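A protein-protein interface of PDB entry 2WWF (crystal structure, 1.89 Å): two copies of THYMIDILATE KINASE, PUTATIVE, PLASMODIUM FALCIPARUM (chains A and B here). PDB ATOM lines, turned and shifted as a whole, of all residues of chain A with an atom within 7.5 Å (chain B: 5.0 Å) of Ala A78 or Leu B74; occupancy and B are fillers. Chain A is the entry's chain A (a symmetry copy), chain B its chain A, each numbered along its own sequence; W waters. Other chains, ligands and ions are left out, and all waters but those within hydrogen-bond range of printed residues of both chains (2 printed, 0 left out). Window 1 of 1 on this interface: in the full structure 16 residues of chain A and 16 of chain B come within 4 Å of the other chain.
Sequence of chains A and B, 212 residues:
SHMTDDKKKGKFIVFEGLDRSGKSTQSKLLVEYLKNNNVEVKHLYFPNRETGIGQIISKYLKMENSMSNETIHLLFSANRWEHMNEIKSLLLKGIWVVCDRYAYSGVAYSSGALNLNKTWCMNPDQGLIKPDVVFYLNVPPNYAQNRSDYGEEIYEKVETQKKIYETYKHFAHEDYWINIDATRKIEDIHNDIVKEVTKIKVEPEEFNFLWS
OG of Ser B77 sits close to O of Pro B124, 3.5 Å away.
The backbone NH (N) of Ile A53 sits close to the side-chain hydroxyl (OG1) of Thr A51 (3.4 Å).
The side-chain hydroxyl (OG1) of Thr A51 lies within hydrogen-bond range of the side-chain carboxylate (OE2) of Glu A82, at 2.7 Å.
The backbone carbonyl oxygen (O) of Pro A124 lies close to the side-chain hydroxyl (OG) of Ser A77 (3.5 Å).
The side-chain carboxylate of Asp A125 sits at hydrogen-bond distance from the side-chain hydroxyl of Ser A77, 2.8 Å away.
OE2 of Glu A82 sits at hydrogen-bond distance from ND2 of Asn A79, at 2.9 Å.
Water W1 lies within hydrogen-bond range of OE1 of Glu B70 (2.8 Å) and O of Trp A81 (3.4 Å).
Water W2 bridges the backbone carbonyl oxygen of Trp B120 and the backbone carbonyl oxygen of Asn A123.
Thr A71 touches Ala B78, and with the chains exchanged Ala A78 touches Thr B71.
Leu A74 touches Ala B78, and with the chains exchanged Ala A78 touches Leu B74.
Leu A74 touches Pro B124, and with the chains exchanged Pro A124 touches Leu B74.
Leu A75 touches its own counterpart, Leu B75.
Of the 20 pairs that touch across the chains among the printed residues, 11 have their exchanged pair printed and touching as well.
Ile A53 touches Thr B71.
Ala B78 touches Thr A71.
CD2 of Leu B75 touches CD2 of Leu A75 (3.6 Å).
Ala B78 touches Leu A75 (CB to CD2, 3.98 Å).
Thr B71 touches Ala A78.
N of Ala A78 touches CD1 of Leu B74 (3.8 Å).
Trp A81 touches Trp B120.
Trp B120 touches Asn A123.
Leu B74 touches Pro A124 (CD2 to CB, 3.7 Å).
Pro A124 touches Trp B120.
Hydrophobic or aromatic side chains of chain A within 4 Å of the printed part of chain B: Ile A53, Leu A74, Leu A75, Ala A78, Trp A81 and Pro A124.
Printed residues of chain B that touch a printed residue of chain A: Glu B70, Thr B71, Leu B74, Leu B75, Ser B77, Ala B78, Trp B120 and Pro B124.
Ala A78 touches three residues of chain B.
Leu B74 touches just these residues of chain A: Ser A77, Ala A78, Trp A81 and Pro A124.
Printed residues of chain B within 4 Å of Trp A81: Glu B70, Thr B71, Leu B74 and Trp B120.
Of the printed residues of chain A, Ala B78 touches Thr A71 (3.7 Å), Leu A74 (3.8 Å) and Leu A75 (3.98 Å).
Of the printed residues of chain A, Ser B77 touches Leu A74.
Ile A57 touches none of the printed residues of chain B.
The nearest residue of chain A that does not touch Leu B74 is Leu A74 (4.2 Å).
The nearest printed residue of chain A that does not touch Trp B120 is Asp A125 (5.2 Å).
The side-chain hydroxyl (OG1) of Thr B71 is in hydrogen-bond range of the backbone NH (N) of Glu A82.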
ATOM      1  N   PHE A  46     -30.202  16.443 -17.273  1.00  0.00           N
ATOM      2  CA  PHE A  46     -29.229  16.136 -16.204  1.00  0.00           C
ATOM      3  C   PHE A  46     -29.949  16.262 -14.854  1.00  0.00           C
ATOM      4  O   PHE A  46     -30.843  17.115 -14.682  1.00  0.00           O
ATOM      5  CB  PHE A  46     -27.994  17.085 -16.313  1.00  0.00           C
ATOM      6  CG  PHE A  46     -27.158  16.798 -17.540  1.00  0.00           C
ATOM      7  CD1 PHE A  46     -26.314  15.674 -17.561  1.00  0.00           C
ATOM      8  CD2 PHE A  46     -27.236  17.588 -18.673  1.00  0.00           C
ATOM      9  CE1 PHE A  46     -25.573  15.362 -18.725  1.00  0.00           C
ATOM     10  CE2 PHE A  46     -26.471  17.283 -19.810  1.00  0.00           C
ATOM     11  CZ  PHE A  46     -25.655  16.200 -19.842  1.00  0.00           C
ATOM     12  N   THR A  51     -26.508   6.223 -15.778  1.00  0.00           N
ATOM     13  CA  THR A  51     -25.089   5.824 -15.861  1.00  0.00           C
ATOM     14  C   THR A  51     -24.648   5.333 -14.460  1.00  0.00           C
ATOM     15  O   THR A  51     -25.356   5.478 -13.473  1.00  0.00           O
ATOM     16  CB  THR A  51     -24.174   7.008 -16.323  1.00  0.00           C
ATOM     17  OG1 THR A  51     -24.080   8.004 -15.262  1.00  0.00           O
ATOM     18  CG2 THR A  51     -24.713   7.655 -17.666  1.00  0.00           C
ATOM     19  N   ILE A  53     -22.347   6.786 -12.603  1.00  0.00           N
ATOM     20  CA  ILE A  53     -22.318   8.009 -11.788  1.00  0.00           C
ATOM     21  C   ILE A  53     -23.757   8.440 -11.448  1.00  0.00           C
ATOM     22  O   ILE A  53     -24.060   8.837 -10.317  1.00  0.00           O
ATOM     23  CB  ILE A  53     -21.578   9.116 -12.581  1.00  0.00           C
ATOM     24  CG1 ILE A  53     -20.085   8.714 -12.682  1.00  0.00           C
ATOM     25  CG2 ILE A  53     -21.794  10.487 -11.899  1.00  0.00           C
ATOM     26  CD1 ILE A  53     -19.380   9.603 -13.842  1.00  0.00           C
ATOM     27  N   ILE A  57     -25.857   9.408  -7.915  1.00  0.00           N
ATOM     28  CA  ILE A  57     -26.594  10.665  -7.789  1.00  0.00           C
ATOM     29  C   ILE A  57     -28.094  10.453  -7.421  1.00  0.00           C
ATOM     30  O   ILE A  57     -28.665  11.117  -6.549  1.00  0.00           O
ATOM     31  CB  ILE A  57     -26.469  11.526  -9.147  1.00  0.00           C
ATOM     32  CG1 ILE A  57     -25.048  12.080  -9.281  1.00  0.00           C
ATOM     33  CG2 ILE A  57     -27.407  12.718  -9.089  1.00  0.00           C
ATOM     34  CD1 ILE A  57     -24.701  12.719 -10.688  1.00  0.00           C
ATOM     35  N   GLU A  70     -18.963  18.427  -1.367  1.00  0.00           N
ATOM     36  CA  GLU A  70     -17.993  18.406  -2.485  1.00  0.00           C
ATOM     37  C   GLU A  70     -18.074  17.166  -3.319  1.00  0.00           C
ATOM     38  O   GLU A  70     -17.945  17.212  -4.560  1.00  0.00           O
ATOM     39  CB  GLU A  70     -16.561  18.541  -1.954  1.00  0.00           C
ATOM     40  CG  GLU A  70     -16.317  19.966  -1.312  1.00  0.00           C
ATOM     41  CD  GLU A  70     -16.739  20.057   0.209  1.00  0.00           C
ATOM     42  OE1 GLU A  70     -17.297  19.089   0.797  1.00  0.00           O
ATOM     43  OE2 GLU A  70     -16.496  21.111   0.795  1.00  0.00           O
ATOM     44  N   THR A  71     -18.249  16.031  -2.658  1.00  0.00           N
ATOM     45  CA  THR A  71     -18.291  14.767  -3.413  1.00  0.00           C
ATOM     46  C   THR A  71     -19.472  14.780  -4.402  1.00  0.00           C
ATOM     47  O   THR A  71     -19.318  14.450  -5.590  1.00  0.00           O
ATOM     48  CB  THR A  71     -18.494  13.533  -2.470  1.00  0.00           C
ATOM     49  OG1 THR A  71     -17.451  13.470  -1.488  1.00  0.00           O
ATOM     50  CG2 THR A  71     -18.467  12.222  -3.240  1.00  0.00           C
ATOM     51  N   ILE A  72     -20.666  15.092  -3.898  1.00  0.00           N
ATOM     52  CA  ILE A  72     -21.856  15.041  -4.807  1.00  0.00           C
ATOM     53  C   ILE A  72     -21.776  16.170  -5.858  1.00  0.00           C
ATOM     54  O   ILE A  72     -22.041  15.916  -7.071  1.00  0.00           O
ATOM     55  CB  ILE A  72     -23.188  15.134  -4.020  1.00  0.00           C
ATOM     56  CG1 ILE A  72     -24.444  14.992  -4.919  1.00  0.00           C
ATOM     57  CG2 ILE A  72     -23.359  16.483  -3.251  1.00  0.00           C
ATOM     58  CD1 ILE A  72     -24.537  13.612  -5.649  1.00  0.00           C
ATOM     59  N   HIS A  73     -21.236  17.338  -5.470  1.00  0.00           N
ATOM     60  CA  HIS A  73     -21.055  18.420  -6.482  1.00  0.00           C
ATOM     61  C   HIS A  73     -20.219  17.927  -7.698  1.00  0.00           C
ATOM     62  O   HIS A  73     -20.527  18.192  -8.891  1.00  0.00           O
ATOM     63  CB  HIS A  73     -20.318  19.631  -5.898  1.00  0.00           C
ATOM     64  CG  HIS A  73     -20.220  20.757  -6.892  1.00  0.00           C
ATOM     65  ND1 HIS A  73     -21.306  21.519  -7.206  1.00  0.00           N
ATOM     66  CD2 HIS A  73     -19.228  21.133  -7.745  1.00  0.00           C
ATOM     67  CE1 HIS A  73     -20.983  22.361  -8.184  1.00  0.00           C
ATOM     68  NE2 HIS A  73     -19.728  22.145  -8.533  1.00  0.00           N
ATOM     69  N   LEU A  74     -19.096  17.274  -7.392  1.00  0.00           N
ATOM     70  CA  LEU A  74     -18.202  16.794  -8.455  1.00  0.00           C
ATOM     71  C   LEU A  74     -18.850  15.648  -9.281  1.00  0.00           C
ATOM     72  O   LEU A  74     -18.610  15.534 -10.484  1.00  0.00           O
ATOM     73  CB  LEU A  74     -16.856  16.360  -7.826  1.00  0.00           C
ATOM     74  CG  LEU A  74     -16.011  17.546  -7.298  1.00  0.00           C
ATOM     75  CD1 LEU A  74     -14.778  16.916  -6.576  1.00  0.00           C
ATOM     76  CD2 LEU A  74     -15.591  18.513  -8.370  1.00  0.00           C
ATOM     77  N   LEU A  75     -19.674  14.795  -8.652  1.00  0.00           N
ATOM     78  CA  LEU A  75     -20.365  13.786  -9.457  1.00  0.00           C
ATOM     79  C   LEU A  75     -21.351  14.424 -10.446  1.00  0.00           C
ATOM     80  O   LEU A  75     -21.543  13.903 -11.559  1.00  0.00           O
ATOM     81  CB  LEU A  75     -21.148  12.771  -8.570  1.00  0.00           C
ATOM     82  CG  LEU A  75     -20.336  11.805  -7.693  1.00  0.00           C
ATOM     83  CD1 LEU A  75     -21.122  10.583  -7.407  1.00  0.00           C
ATOM     84  CD2 LEU A  75     -19.021  11.398  -8.358  1.00  0.00           C
ATOM     85  N   PHE A  76     -22.038  15.496 -10.012  1.00  0.00           N
ATOM     86  CA  PHE A  76     -23.030  16.156 -10.926  1.00  0.00           C
ATOM     87  C   PHE A  76     -22.286  16.698 -12.153  1.00  0.00           C
ATOM     88  O   PHE A  76     -22.747  16.553 -13.332  1.00  0.00           O
ATOM     89  CB  PHE A  76     -23.748  17.293 -10.225  1.00  0.00           C
ATOM     90  CG  PHE A  76     -25.026  16.888  -9.525  1.00  0.00           C
ATOM     91  CD1 PHE A  76     -26.153  16.452 -10.276  1.00  0.00           C
ATOM     92  CD2 PHE A  76     -25.148  17.015  -8.139  1.00  0.00           C
ATOM     93  CE1 PHE A  76     -27.417  16.158  -9.633  1.00  0.00           C
ATOM     94  CE2 PHE A  76     -26.379  16.690  -7.510  1.00  0.00           C
ATOM     95  CZ  PHE A  76     -27.514  16.258  -8.271  1.00  0.00           C
ATOM     96  N   SER A  77     -21.102  17.241 -11.914  1.00  0.00           N
ATOM     97  CA  SER A  77     -20.244  17.707 -13.029  1.00  0.00           C
ATOM     98  C   SER A  77     -19.701  16.560 -13.944  1.00  0.00           C
ATOM     99  O   SER A  77     -19.762  16.619 -15.192  1.00  0.00           O
ATOM    100  CB  SER A  77     -19.071  18.528 -12.472  1.00  0.00           C
ATOM    101  OG  SER A  77     -18.352  19.025 -13.611  1.00  0.00           O
ATOM    102  N   ALA A  78     -19.143  15.525 -13.320  1.00  0.00           N
ATOM    103  CA  ALA A  78     -18.658  14.352 -14.067  1.00  0.00           C
ATOM    104  C   ALA A  78     -19.793  13.734 -14.930  1.00  0.00           C
ATOM    105  O   ALA A  78     -19.527  13.228 -15.998  1.00  0.00           O
ATOM    106  CB  ALA A  78     -18.170  13.334 -13.076  1.00  0.00           C
ATOM    107  N   ASN A  79     -21.014  13.727 -14.396  1.00  0.00           N
ATOM    108  CA  ASN A  79     -22.205  13.230 -15.132  1.00  0.00           C
ATOM    109  C   ASN A  79     -22.452  14.006 -16.440  1.00  0.00           C
ATOM    110  O   ASN A  79     -22.822  13.406 -17.469  1.00  0.00           O
ATOM    111  CB  ASN A  79     -23.430  13.364 -14.241  1.00  0.00           C
ATOM    112  CG  ASN A  79     -24.695  12.682 -14.808  1.00  0.00           C
ATOM    113  OD1 ASN A  79     -25.771  13.271 -14.731  1.00  0.00           O
ATOM    114  ND2 ASN A  79     -24.585  11.408 -15.248  1.00  0.00           N
ATOM    115  N   ARG A  80     -22.223  15.310 -16.414  1.00  0.00           N
ATOM    116  CA  ARG A  80     -22.213  16.126 -17.687  1.00  0.00           C
ATOM    117  C   ARG A  80     -21.060  15.799 -18.612  1.00  0.00           C
ATOM    118  O   ARG A  80     -21.260  15.639 -19.823  1.00  0.00           O
ATOM    119  CB  ARG A  80     -22.205  17.630 -17.393  1.00  0.00           C
ATOM    120  CG  ARG A  80     -23.594  18.122 -16.822  1.00  0.00           C
ATOM    121  CD  ARG A  80     -23.600  19.610 -16.563  1.00  0.00           C
ATOM    122  NE  ARG A  80     -22.883  19.983 -15.334  1.00  0.00           N
ATOM    123  CZ  ARG A  80     -23.392  19.838 -14.089  1.00  0.00           C
ATOM    124  NH1 ARG A  80     -24.567  19.255 -13.893  1.00  0.00           N
ATOM    125  NH2 ARG A  80     -22.753  20.320 -13.034  1.00  0.00           N
ATOM    126  N   TRP A  81     -19.842  15.698 -18.070  1.00  0.00           N
ATOM    127  CA  TRP A  81     -18.715  15.381 -18.914  1.00  0.00           C
ATOM    128  C   TRP A  81     -18.893  14.088 -19.687  1.00  0.00           C
ATOM    129  O   TRP A  81     -18.443  13.967 -20.847  1.00  0.00           O
ATOM    130  CB  TRP A  81     -17.419  15.337 -18.058  1.00  0.00           C
ATOM    131  CG  TRP A  81     -16.896  16.764 -17.818  1.00  0.00           C
ATOM    132  CD1 TRP A  81     -16.938  17.514 -16.655  1.00  0.00           C
ATOM    133  CD2 TRP A  81     -16.236  17.582 -18.799  1.00  0.00           C
ATOM    134  NE1 TRP A  81     -16.392  18.760 -16.880  1.00  0.00           N
ATOM    135  CE2 TRP A  81     -15.893  18.802 -18.162  1.00  0.00           C
ATOM    136  CE3 TRP A  81     -15.881  17.379 -20.159  1.00  0.00           C
ATOM    137  CZ2 TRP A  81     -15.265  19.862 -18.841  1.00  0.00           C
ATOM    138  CZ3 TRP A  81     -15.236  18.445 -20.848  1.00  0.00           C
ATOM    139  CH2 TRP A  81     -14.917  19.653 -20.161  1.00  0.00           C
ATOM    140  N   GLU A  82     -19.473  13.073 -19.053  1.00  0.00           N
ATOM    141  CA  GLU A  82     -19.561  11.775 -19.766  1.00  0.00           C
ATOM    142  C   GLU A  82     -20.575  11.837 -20.938  1.00  0.00           C
ATOM    143  O   GLU A  82     -20.707  10.861 -21.749  1.00  0.00           O
ATOM    144  CB  GLU A  82     -19.899  10.641 -18.782  1.00  0.00           C
ATOM    145  CG  GLU A  82     -21.302  10.704 -18.138  1.00  0.00           C
ATOM    146  CD  GLU A  82     -21.547   9.589 -17.047  1.00  0.00           C
ATOM    147  OE1 GLU A  82     -20.972   8.447 -17.120  1.00  0.00           O
ATOM    148  OE2 GLU A  82     -22.346   9.807 -16.139  1.00  0.00           O
ATOM    149  N   HIS A  83     -21.266  12.967 -21.047  1.00  0.00           N
ATOM    150  CA  HIS A  83     -22.152  13.242 -22.202  1.00  0.00           C
ATOM    151  C   HIS A  83     -21.568  14.156 -23.247  1.00  0.00           C
ATOM    152  O   HIS A  83     -22.261  14.393 -24.268  1.00  0.00           O
ATOM    153  CB  HIS A  83     -23.500  13.866 -21.760  1.00  0.00           C
ATOM    154  CG  HIS A  83     -24.346  12.886 -20.994  1.00  0.00           C
ATOM    155  ND1 HIS A  83     -23.975  12.457 -19.731  1.00  0.00           N
ATOM    156  CD2 HIS A  83     -25.409  12.127 -21.351  1.00  0.00           C
ATOM    157  CE1 HIS A  83     -24.813  11.523 -19.308  1.00  0.00           C
ATOM    158  NE2 HIS A  83     -25.705  11.309 -20.270  1.00  0.00           N
ATOM    159  N   MET A  84     -20.383  14.725 -23.016  1.00  0.00           N
ATOM    160  CA  MET A  84     -19.812  15.622 -24.032  1.00  0.00           C
ATOM    161  C   MET A  84     -19.559  15.035 -25.418  1.00  0.00           C
ATOM    162  O   MET A  84     -19.764  15.757 -26.419  1.00  0.00           O
ATOM    163  CB  MET A  84     -18.576  16.375 -23.543  1.00  0.00           C
ATOM    164  CG  MET A  84     -18.932  17.400 -22.448  1.00  0.00           C
ATOM    165  SD  MET A  84     -20.097  18.732 -23.006  1.00  0.00           S
ATOM    166  CE  MET A  84     -21.663  18.176 -22.274  1.00  0.00           C
ATOM    167  N   ASN A 123     -15.731  25.753 -11.353  1.00  0.00           N
ATOM    168  CA  ASN A 123     -14.492  25.200 -11.967  1.00  0.00           C
ATOM    169  C   ASN A 123     -14.598  23.883 -12.728  1.00  0.00           C
ATOM    170  O   ASN A 123     -14.038  23.804 -13.821  1.00  0.00           O
ATOM    171  CB  ASN A 123     -13.361  25.119 -10.954  1.00  0.00           C
ATOM    172  CG  ASN A 123     -12.815  26.520 -10.553  1.00  0.00           C
ATOM    173  OD1 ASN A 123     -12.931  27.501 -11.299  1.00  0.00           O
ATOM    174  ND2 ASN A 123     -12.242  26.596  -9.356  1.00  0.00           N
ATOM    175  N   PRO A 124     -15.221  22.821 -12.122  1.00  0.00           N
ATOM    176  CA  PRO A 124     -15.162  21.535 -12.820  1.00  0.00           C
ATOM    177  C   PRO A 124     -16.000  21.546 -14.102  1.00  0.00           C
ATOM    178  O   PRO A 124     -15.667  20.793 -14.978  1.00  0.00           O
ATOM    179  CB  PRO A 124     -15.770  20.501 -11.798  1.00  0.00           C
ATOM    180  CG  PRO A 124     -16.632  21.333 -10.907  1.00  0.00           C
ATOM    181  CD  PRO A 124     -15.781  22.657 -10.766  1.00  0.00           C
ATOM    182  N   ASP A 125     -17.016  22.432 -14.218  1.00  0.00           N
ATOM    183  CA  ASP A 125     -17.794  22.563 -15.489  1.00  0.00           C
ATOM    184  C   ASP A 125     -17.147  23.465 -16.558  1.00  0.00           C
ATOM    185  O   ASP A 125     -17.634  23.529 -17.711  1.00  0.00           O
ATOM    186  CB  ASP A 125     -19.165  23.126 -15.141  1.00  0.00           C
ATOM    187  CG  ASP A 125     -20.089  22.059 -14.521  1.00  0.00           C
ATOM    188  OD1 ASP A 125     -19.939  20.865 -14.911  1.00  0.00           O
ATOM    189  OD2 ASP A 125     -20.976  22.423 -13.739  1.00  0.00           O
ATOM    190  N   LEU A 128     -17.028  22.561 -20.623  1.00  0.00           N
ATOM    191  CA  LEU A 128     -18.263  21.931 -21.199  1.00  0.00           C
ATOM    192  C   LEU A 128     -18.744  22.790 -22.393  1.00  0.00           C
ATOM    193  O   LEU A 128     -18.458  23.960 -22.437  1.00  0.00           O
ATOM    194  CB  LEU A 128     -19.413  21.867 -20.204  1.00  0.00           C
ATOM    195  CG  LEU A 128     -19.222  20.909 -18.976  1.00  0.00           C
ATOM    196  CD1 LEU A 128     -20.485  21.038 -18.073  1.00  0.00           C
ATOM    197  CD2 LEU A 128     -18.997  19.412 -19.430  1.00  0.00           C
ATOM    198  N   GLU B  70     -11.948  13.984 -18.693  1.00  0.00           N
ATOM    199  CA  GLU B  70     -12.535  14.833 -17.633  1.00  0.00           C
ATOM    200  C   GLU B  70     -13.379  14.071 -16.660  1.00  0.00           C
ATOM    201  O   GLU B  70     -13.362  14.340 -15.442  1.00  0.00           O
ATOM    202  CB  GLU B  70     -13.390  15.945 -18.251  1.00  0.00           C
ATOM    203  CG  GLU B  70     -12.502  16.972 -19.063  1.00  0.00           C
ATOM    204  CD  GLU B  70     -12.238  16.537 -20.560  1.00  0.00           C
ATOM    205  OE1 GLU B  70     -12.641  15.426 -21.003  1.00  0.00           O
ATOM    206  OE2 GLU B  70     -11.627  17.331 -21.274  1.00  0.00           O
ATOM    207  N   THR B  71     -14.161  13.135 -17.178  1.00  0.00           N
ATOM    208  CA  THR B  71     -15.052  12.378 -16.282  1.00  0.00           C
ATOM    209  C   THR B  71     -14.223  11.604 -15.241  1.00  0.00           C
ATOM    210  O   THR B  71     -14.512  11.645 -14.032  1.00  0.00           O
ATOM    211  CB  THR B  71     -15.906  11.325 -17.067  1.00  0.00           C
ATOM    212  OG1 THR B  71     -16.683  11.964 -18.089  1.00  0.00           O
ATOM    213  CG2 THR B  71     -16.877  10.592 -16.155  1.00  0.00           C
ATOM    214  N   ILE B  72     -13.238  10.841 -15.713  1.00  0.00           N
ATOM    215  CA  ILE B  72     -12.456  10.008 -14.743  1.00  0.00           C
ATOM    216  C   ILE B  72     -11.596  10.913 -13.833  1.00  0.00           C
ATOM    217  O   ILE B  72     -11.553  10.687 -12.587  1.00  0.00           O
ATOM    218  CB  ILE B  72     -11.561   8.969 -15.465  1.00  0.00           C
ATOM    219  CG1 ILE B  72     -10.806   8.027 -14.491  1.00  0.00           C
ATOM    220  CG2 ILE B  72     -10.467   9.616 -16.372  1.00  0.00           C
ATOM    221  CD1 ILE B  72     -11.754   7.154 -13.604  1.00  0.00           C
ATOM    222  N   HIS B  73     -11.082  12.029 -14.379  1.00  0.00           N
ATOM    223  CA  HIS B  73     -10.324  12.975 -13.508  1.00  0.00           C
ATOM    224  C   HIS B  73     -11.178  13.432 -12.289  1.00  0.00           C
ATOM    225  O   HIS B  73     -10.715  13.503 -11.120  1.00  0.00           O
ATOM    226  CB  HIS B  73      -9.915  14.244 -14.265  1.00  0.00           C
ATOM    227  CG  HIS B  73      -9.073  15.154 -13.411  1.00  0.00           C
ATOM    228  ND1 HIS B  73      -7.773  14.855 -13.129  1.00  0.00           N
ATOM    229  CD2 HIS B  73      -9.387  16.245 -12.660  1.00  0.00           C
ATOM    230  CE1 HIS B  73      -7.293  15.752 -12.272  1.00  0.00           C
ATOM    231  NE2 HIS B  73      -8.253  16.605 -11.967  1.00  0.00           N
ATOM    232  N   LEU B  74     -12.419  13.829 -12.578  1.00  0.00           N
ATOM    233  CA  LEU B  74     -13.308  14.320 -11.516  1.00  0.00           C
ATOM    234  C   LEU B  74     -13.712  13.188 -10.532  1.00  0.00           C
ATOM    235  O   LEU B  74     -13.892  13.433  -9.338  1.00  0.00           O
ATOM    236  CB  LEU B  74     -14.545  14.992 -12.161  1.00  0.00           C
ATOM    237  CG  LEU B  74     -14.221  16.333 -12.864  1.00  0.00           C
ATOM    238  CD1 LEU B  74     -15.537  16.782 -13.574  1.00  0.00           C
ATOM    239  CD2 LEU B  74     -13.704  17.394 -11.933  1.00  0.00           C
ATOM    240  N   LEU B  75     -13.857  11.944 -11.015  1.00  0.00           N
ATOM    241  CA  LEU B  75     -14.131  10.864 -10.066  1.00  0.00           C
ATOM    242  C   LEU B  75     -12.955  10.638  -9.105  1.00  0.00           C
ATOM    243  O   LEU B  75     -13.167  10.285  -7.932  1.00  0.00           O
ATOM    244  CB  LEU B  75     -14.440   9.517 -10.788  1.00  0.00           C
ATOM    245  CG  LEU B  75     -15.746   9.413 -11.591  1.00  0.00           C
ATOM    246  CD1 LEU B  75     -16.177   8.001 -11.695  1.00  0.00           C
ATOM    247  CD2 LEU B  75     -16.874  10.226 -10.955  1.00  0.00           C
ATOM    248  N   PHE B  76     -11.719  10.755  -9.621  1.00  0.00           N
ATOM    249  CA  PHE B  76     -10.525  10.530  -8.737  1.00  0.00           C
ATOM    250  C   PHE B  76     -10.533  11.582  -7.621  1.00  0.00           C
ATOM    251  O   PHE B  76     -10.282  11.273  -6.410  1.00  0.00           O
ATOM    252  CB  PHE B  76      -9.234  10.634  -9.525  1.00  0.00           C
ATOM    253  CG  PHE B  76      -8.748   9.327 -10.106  1.00  0.00           C
ATOM    254  CD1 PHE B  76      -8.307   8.277  -9.251  1.00  0.00           C
ATOM    255  CD2 PHE B  76      -8.645   9.158 -11.489  1.00  0.00           C
ATOM    256  CE1 PHE B  76      -7.742   7.057  -9.790  1.00  0.00           C
ATOM    257  CE2 PHE B  76      -8.126   7.943 -12.011  1.00  0.00           C
ATOM    258  CZ  PHE B  76      -7.676   6.892 -11.148  1.00  0.00           C
ATOM    259  N   SER B  77     -10.904  12.801  -7.983  1.00  0.00           N
ATOM    260  CA  SER B  77     -11.048  13.877  -6.974  1.00  0.00           C
ATOM    261  C   SER B  77     -12.222  13.658  -5.965  1.00  0.00           C
ATOM    262  O   SER B  77     -12.072  13.792  -4.730  1.00  0.00           O
ATOM    263  CB  SER B  77     -11.216  15.231  -7.682  1.00  0.00           C
ATOM    264  OG  SER B  77     -11.247  16.225  -6.646  1.00  0.00           O
ATOM    265  N   ALA B  78     -13.403  13.346  -6.495  1.00  0.00           N
ATOM    266  CA  ALA B  78     -14.568  13.046  -5.647  1.00  0.00           C
ATOM    267  C   ALA B  78     -14.255  11.887  -4.660  1.00  0.00           C
ATOM    268  O   ALA B  78     -14.755  11.886  -3.557  1.00  0.00           O
ATOM    269  CB  ALA B  78     -15.710  12.651  -6.539  1.00  0.00           C
ATOM    270  N   ASN B  79     -13.495  10.896  -5.124  1.00  0.00           N
ATOM    271  CA  ASN B  79     -13.060   9.758  -4.275  1.00  0.00           C
ATOM    272  C   ASN B  79     -12.242  10.216  -3.052  1.00  0.00           C
ATOM    273  O   ASN B  79     -12.402   9.668  -1.944  1.00  0.00           O
ATOM    274  CB  ASN B  79     -12.209   8.812  -5.110  1.00  0.00           C
ATOM    275  CG  ASN B  79     -11.875   7.480  -4.403  1.00  0.00           C
ATOM    276  OD1 ASN B  79     -10.734   7.032  -4.490  1.00  0.00           O
ATOM    277  ND2 ASN B  79     -12.890   6.795  -3.827  1.00  0.00           N
ATOM    278  N   TRP B 120      -6.763  23.320 -14.546  1.00  0.00           N
ATOM    279  CA  TRP B 120      -8.078  22.606 -14.503  1.00  0.00           C
ATOM    280  C   TRP B 120      -8.006  21.333 -13.622  1.00  0.00           C
ATOM    281  O   TRP B 120      -8.953  21.045 -12.853  1.00  0.00           O
ATOM    282  CB  TRP B 120      -8.511  22.270 -15.952  1.00  0.00           C
ATOM    283  CG  TRP B 120      -9.956  21.792 -15.999  1.00  0.00           C
ATOM    284  CD1 TRP B 120     -11.065  22.579 -16.156  1.00  0.00           C
ATOM    285  CD2 TRP B 120     -10.435  20.428 -15.868  1.00  0.00           C
ATOM    286  NE1 TRP B 120     -12.196  21.786 -16.125  1.00  0.00           N
ATOM    287  CE2 TRP B 120     -11.838  20.469 -15.975  1.00  0.00           C
ATOM    288  CE3 TRP B 120      -9.806  19.179 -15.717  1.00  0.00           C
ATOM    289  CZ2 TRP B 120     -12.641  19.303 -15.900  1.00  0.00           C
ATOM    290  CZ3 TRP B 120     -10.626  17.998 -15.604  1.00  0.00           C
ATOM    291  CH2 TRP B 120     -12.017  18.096 -15.697  1.00  0.00           C
ATOM    292  N   PRO B 124     -10.479  20.865  -8.720  1.00  0.00           N
ATOM    293  CA  PRO B 124     -11.456  20.165  -7.884  1.00  0.00           C
ATOM    294  C   PRO B 124     -10.836  19.682  -6.570  1.00  0.00           C
ATOM    295  O   PRO B 124     -11.578  19.551  -5.632  1.00  0.00           O
ATOM    296  CB  PRO B 124     -11.898  18.924  -8.749  1.00  0.00           C
ATOM    297  CG  PRO B 124     -10.755  18.703  -9.682  1.00  0.00           C
ATOM    298  CD  PRO B 124     -10.311  20.182 -10.018  1.00  0.00           C
HETATM  299  O   HOH W   1     -15.207  14.531 -21.594  1.00  0.00           O
HETATM  300  O   HOH W   2     -11.589  22.324 -12.926  1.00  0.00           O
